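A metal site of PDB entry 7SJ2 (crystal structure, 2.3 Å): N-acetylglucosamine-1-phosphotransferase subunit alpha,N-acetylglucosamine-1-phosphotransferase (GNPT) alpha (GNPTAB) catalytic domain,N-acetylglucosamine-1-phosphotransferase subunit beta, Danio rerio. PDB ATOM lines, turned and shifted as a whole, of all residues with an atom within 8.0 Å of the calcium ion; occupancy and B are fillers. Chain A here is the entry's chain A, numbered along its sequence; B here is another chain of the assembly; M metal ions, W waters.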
ATOM      1  N   PHE A 301       1.810 -11.509  21.963  1.00  0.00           N
ATOM      2  CA  PHE A 301       2.437 -10.319  21.398  1.00  0.00           C
ATOM      3  C   PHE A 301       3.416 -10.677  20.293  1.00  0.00           C
ATOM      4  O   PHE A 301       3.414 -10.052  19.227  1.00  0.00           O
ATOM      5  CB  PHE A 301       3.144  -9.547  22.521  1.00  0.00           C
ATOM      6  CG  PHE A 301       3.722  -8.249  22.084  1.00  0.00           C
ATOM      7  CD1 PHE A 301       4.997  -8.177  21.561  1.00  0.00           C
ATOM      8  CD2 PHE A 301       2.987  -7.076  22.219  1.00  0.00           C
ATOM      9  CE1 PHE A 301       5.525  -6.972  21.156  1.00  0.00           C
ATOM     10  CE2 PHE A 301       3.515  -5.868  21.824  1.00  0.00           C
ATOM     11  CZ  PHE A 301       4.792  -5.812  21.295  1.00  0.00           C
ATOM     12  N   ILE A 304       1.655 -11.523  17.103  1.00  0.00           N
ATOM     13  CA  ILE A 304       1.089 -10.344  16.464  1.00  0.00           C
ATOM     14  C   ILE A 304       2.192  -9.498  15.837  1.00  0.00           C
ATOM     15  O   ILE A 304       2.027  -8.944  14.747  1.00  0.00           O
ATOM     16  CB  ILE A 304       0.256  -9.533  17.473  1.00  0.00           C
ATOM     17  CG1 ILE A 304      -0.768 -10.427  18.193  1.00  0.00           C
ATOM     18  CG2 ILE A 304      -0.455  -8.380  16.791  1.00  0.00           C
ATOM     19  CD1 ILE A 304      -1.797 -11.059  17.282  1.00  0.00           C
ATOM     20  N   ASP A 305       3.338  -9.382  16.525  1.00  0.00           N
ATOM     21  CA  ASP A 305       4.454  -8.547  16.084  1.00  0.00           C
ATOM     22  C   ASP A 305       5.225  -9.296  15.007  1.00  0.00           C
ATOM     23  O   ASP A 305       6.312  -9.838  15.218  1.00  0.00           O
ATOM     24  CB  ASP A 305       5.335  -8.196  17.285  1.00  0.00           C
ATOM     25  CG  ASP A 305       6.484  -7.279  16.926  1.00  0.00           C
ATOM     26  OD1 ASP A 305       6.232  -6.244  16.273  1.00  0.00           O
ATOM     27  OD2 ASP A 305       7.628  -7.578  17.318  1.00  0.00           O
ATOM     28  N   THR A 306       4.646  -9.307  13.804  1.00  0.00           N
ATOM     29  CA  THR A 306       5.153 -10.170  12.735  1.00  0.00           C
ATOM     30  C   THR A 306       6.476  -9.681  12.144  1.00  0.00           C
ATOM     31  O   THR A 306       7.181 -10.488  11.530  1.00  0.00           O
ATOM     32  CB  THR A 306       4.105 -10.286  11.622  1.00  0.00           C
ATOM     33  OG1 THR A 306       3.644  -8.978  11.264  1.00  0.00           O
ATOM     34  CG2 THR A 306       2.924 -11.145  12.082  1.00  0.00           C
ATOM     35  N   ASP A 307       6.821  -8.401  12.311  1.00  0.00           N
ATOM     36  CA  ASP A 307       8.135  -7.920  11.907  1.00  0.00           C
ATOM     37  C   ASP A 307       9.163  -8.017  13.039  1.00  0.00           C
ATOM     38  O   ASP A 307      10.322  -7.617  12.841  1.00  0.00           O
ATOM     39  CB  ASP A 307       8.052  -6.471  11.407  1.00  0.00           C
ATOM     40  CG  ASP A 307       7.545  -5.499  12.457  1.00  0.00           C
ATOM     41  OD1 ASP A 307       7.411  -5.894  13.641  1.00  0.00           O
ATOM     42  OD2 ASP A 307       7.278  -4.336  12.103  1.00  0.00           O
ATOM     43  N   HIS A 308       8.772  -8.534  14.200  1.00  0.00           N
ATOM     44  CA  HIS A 308       9.678  -8.729  15.334  1.00  0.00           C
ATOM     45  C   HIS A 308      10.330  -7.416  15.765  1.00  0.00           C
ATOM     46  O   HIS A 308      11.491  -7.406  16.199  1.00  0.00           O
ATOM     47  CB  HIS A 308      10.755  -9.770  15.011  1.00  0.00           C
ATOM     48  CG  HIS A 308      10.238 -10.938  14.234  1.00  0.00           C
ATOM     49  ND1 HIS A 308       9.123 -11.654  14.598  1.00  0.00           N
ATOM     50  CD2 HIS A 308      10.700 -11.527  13.101  1.00  0.00           C
ATOM     51  CE1 HIS A 308       8.913 -12.619  13.731  1.00  0.00           C
ATOM     52  NE2 HIS A 308       9.865 -12.567  12.811  1.00  0.00           N
ATOM     53  N   SER A 309       9.612  -6.306  15.662  1.00  0.00           N
ATOM     54  CA  SER A 309      10.150  -5.000  15.995  1.00  0.00           C
ATOM     55  C   SER A 309       9.905  -4.603  17.447  1.00  0.00           C
ATOM     56  O   SER A 309      10.385  -3.541  17.870  1.00  0.00           O
ATOM     57  CB  SER A 309       9.548  -3.934  15.070  1.00  0.00           C
ATOM     58  OG  SER A 309       8.193  -3.696  15.392  1.00  0.00           O
ATOM     59  N   GLY A 310       9.193  -5.413  18.218  1.00  0.00           N
ATOM     60  CA  GLY A 310       8.891  -5.078  19.595  1.00  0.00           C
ATOM     61  C   GLY A 310       7.830  -4.016  19.767  1.00  0.00           C
ATOM     62  O   GLY A 310       7.438  -3.744  20.911  1.00  0.00           O
ATOM     63  N   VAL A 311       7.350  -3.395  18.689  1.00  0.00           N
ATOM     64  CA  VAL A 311       6.268  -2.420  18.735  1.00  0.00           C
ATOM     65  C   VAL A 311       5.173  -2.882  17.781  1.00  0.00           C
ATOM     66  O   VAL A 311       5.462  -3.416  16.707  1.00  0.00           O
ATOM     67  CB  VAL A 311       6.759  -1.008  18.355  1.00  0.00           C
ATOM     68  CG1 VAL A 311       5.600  -0.017  18.321  1.00  0.00           C
ATOM     69  CG2 VAL A 311       7.837  -0.551  19.325  1.00  0.00           C
ATOM     70  N   LEU A 312       3.923  -2.692  18.180  1.00  0.00           N
ATOM     71  CA  LEU A 312       2.785  -3.092  17.350  1.00  0.00           C
ATOM     72  C   LEU A 312       2.367  -1.920  16.476  1.00  0.00           C
ATOM     73  O   LEU A 312       1.973  -0.869  16.982  1.00  0.00           O
ATOM     74  CB  LEU A 312       1.617  -3.563  18.202  1.00  0.00           C
ATOM     75  CG  LEU A 312       1.831  -4.816  19.051  1.00  0.00           C
ATOM     76  CD1 LEU A 312       0.504  -5.292  19.638  1.00  0.00           C
ATOM     77  CD2 LEU A 312       2.509  -5.945  18.272  1.00  0.00           C
ATOM     78  N   SER A 313       2.475  -2.101  15.168  1.00  0.00           N
ATOM     79  CA  SER A 313       1.951  -1.121  14.231  1.00  0.00           C
ATOM     80  C   SER A 313       0.419  -1.187  14.209  1.00  0.00           C
ATOM     81  O   SER A 313      -0.200  -2.108  14.747  1.00  0.00           O
ATOM     82  CB  SER A 313       2.522  -1.375  12.836  1.00  0.00           C
ATOM     83  OG  SER A 313       2.150  -2.666  12.364  1.00  0.00           O
ATOM     84  N   ASP A 314      -0.190  -0.183  13.578  1.00  0.00           N
ATOM     85  CA  ASP A 314      -1.636  -0.216  13.369  1.00  0.00           C
ATOM     86  C   ASP A 314      -2.044  -1.503  12.663  1.00  0.00           C
ATOM     87  O   ASP A 314      -3.051  -2.127  13.020  1.00  0.00           O
ATOM     88  CB  ASP A 314      -2.077   1.002  12.556  1.00  0.00           C
ATOM     89  CG  ASP A 314      -1.885   2.311  13.297  1.00  0.00           C
ATOM     90  OD1 ASP A 314      -2.087   2.337  14.527  1.00  0.00           O
ATOM     91  OD2 ASP A 314      -1.534   3.319  12.637  1.00  0.00           O
ATOM     92  N   GLU A 316      -0.590  -4.422  12.720  1.00  0.00           N
ATOM     93  CA  GLU A 316      -0.534  -5.536  13.660  1.00  0.00           C
ATOM     94  C   GLU A 316      -1.598  -5.405  14.745  1.00  0.00           C
ATOM     95  O   GLU A 316      -2.155  -6.410  15.197  1.00  0.00           O
ATOM     96  CB  GLU A 316       0.858  -5.622  14.279  1.00  0.00           C
ATOM     97  CG  GLU A 316       1.958  -5.964  13.269  1.00  0.00           C
ATOM     98  CD  GLU A 316       3.360  -5.645  13.766  1.00  0.00           C
ATOM     99  OE1 GLU A 316       3.502  -4.830  14.711  1.00  0.00           O
ATOM    100  OE2 GLU A 316       4.320  -6.195  13.211  1.00  0.00           O
ATOM    101  N   ILE A 317      -1.899  -4.169  15.145  1.00  0.00           N
ATOM    102  CA  ILE A 317      -2.939  -3.955  16.163  1.00  0.00           C
ATOM    103  C   ILE A 317      -4.282  -4.461  15.662  1.00  0.00           C
ATOM    104  O   ILE A 317      -5.082  -5.002  16.431  1.00  0.00           O
ATOM    105  CB  ILE A 317      -3.002  -2.464  16.539  1.00  0.00           C
ATOM    106  CG1 ILE A 317      -1.922  -2.143  17.581  1.00  0.00           C
ATOM    107  CG2 ILE A 317      -4.384  -2.091  17.074  1.00  0.00           C
ATOM    108  CD1 ILE A 317      -1.555  -0.679  17.622  1.00  0.00           C
ATOM    109  N   GLU A 363       7.514   3.991  15.170  1.00  0.00           N
ATOM    110  CA  GLU A 363       6.212   3.601  14.641  1.00  0.00           C
ATOM    111  C   GLU A 363       5.371   4.849  14.375  1.00  0.00           C
ATOM    112  O   GLU A 363       5.287   5.743  15.217  1.00  0.00           O
ATOM    113  CB  GLU A 363       5.498   2.686  15.624  1.00  0.00           C
ATOM    114  CG  GLU A 363       4.378   1.860  14.994  1.00  0.00           C
ATOM    115  CD  GLU A 363       4.893   0.869  13.971  1.00  0.00           C
ATOM    116  OE1 GLU A 363       5.753   0.032  14.328  1.00  0.00           O
ATOM    117  OE2 GLU A 363       4.456   0.935  12.805  1.00  0.00           O
ATOM    118  N   TYR A 365       1.710   6.052  13.812  1.00  0.00           N
ATOM    119  CA  TYR A 365       0.348   5.622  14.063  1.00  0.00           C
ATOM    120  C   TYR A 365      -0.660   6.561  13.431  1.00  0.00           C
ATOM    121  O   TYR A 365      -0.399   7.754  13.245  1.00  0.00           O
ATOM    122  CB  TYR A 365       0.080   5.529  15.574  1.00  0.00           C
ATOM    123  CG  TYR A 365       0.856   4.444  16.275  1.00  0.00           C
ATOM    124  CD1 TYR A 365       0.449   3.116  16.189  1.00  0.00           C
ATOM    125  CD2 TYR A 365       1.988   4.729  17.020  1.00  0.00           C
ATOM    126  CE1 TYR A 365       1.150   2.110  16.839  1.00  0.00           C
ATOM    127  CE2 TYR A 365       2.695   3.735  17.675  1.00  0.00           C
ATOM    128  CZ  TYR A 365       2.267   2.427  17.574  1.00  0.00           C
ATOM    129  OH  TYR A 365       2.972   1.426  18.211  1.00  0.00           O
ATOM    130  N   VAL A 373       3.388   1.059  21.027  1.00  0.00           N
ATOM    131  CA  VAL A 373       2.752  -0.099  21.646  1.00  0.00           C
ATOM    132  C   VAL A 373       3.784  -1.191  21.857  1.00  0.00           C
ATOM    133  O   VAL A 373       3.915  -2.118  21.042  1.00  0.00           O
ATOM    134  CB  VAL A 373       1.567  -0.595  20.794  1.00  0.00           C
ATOM    135  CG1 VAL A 373       0.896  -1.803  21.449  1.00  0.00           C
ATOM    136  CG2 VAL A 373       0.567   0.525  20.579  1.00  0.00           C
ATOM    137  N   PRO B 464       5.658  -9.386   6.653  1.00  0.00           N
ATOM    138  CA  PRO B 464       6.297  -8.106   6.343  1.00  0.00           C
ATOM    139  C   PRO B 464       7.778  -8.203   6.035  1.00  0.00           C
ATOM    140  O   PRO B 464       8.350  -7.219   5.534  1.00  0.00           O
ATOM    141  CB  PRO B 464       6.064  -7.289   7.625  1.00  0.00           C
ATOM    142  CG  PRO B 464       6.077  -8.321   8.703  1.00  0.00           C
ATOM    143  CD  PRO B 464       5.449  -9.563   8.100  1.00  0.00           C
HETATM  144 CA    CA M   1       5.943  -4.604  14.793  1.00  0.00          CA
HETATM  145  O   HOH W   1       5.632  -2.747  13.267  1.00  0.00           O
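The backbone NH (N) of Thr 306 lies close to the side-chain carboxylate (OE2) of Glu 316. The side-chain hydroxyl (OG) of Ser 313 lies within hydrogen-bond range of the backbone NH (N) of Glu 316 (3.3 Å). The backbone NH (N) of Gly 310 sits at hydrogen-bond distance from the side-chain carboxylate (OD2) of Asp 305, 2.8 Å away. The backbone carbonyl oxygen (O) of Asp 305 lies within hydrogen-bond range of a ring nitrogen (ND1) of His 308, at 3.4 Å.
The nearest printed residue that does not touch the calcium ion is Ser 313 (4.3 Å).
The calcium ion is bound by OD1 of Asp 305 (2.2 Å), OD1 of Asp 307 (2.3 Å), O of Val 311 (2.3 Å), water W1 (2.4 Å), OE1 of Glu 316 (2.5 Å), OG of Ser 309 (2.5 Å) and OE2 of Glu 316 (2.8 Å). Slightly farther from the calcium ion lies the side-chain carboxylate (OD2) of Asp 307 (3.0 Å).
Water W1 bridges the side-chain carboxylate (OD2) of Asp 307 (2.6 Å) and the side-chain carboxylate (OE1) of Glu 363 (3.0 Å).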
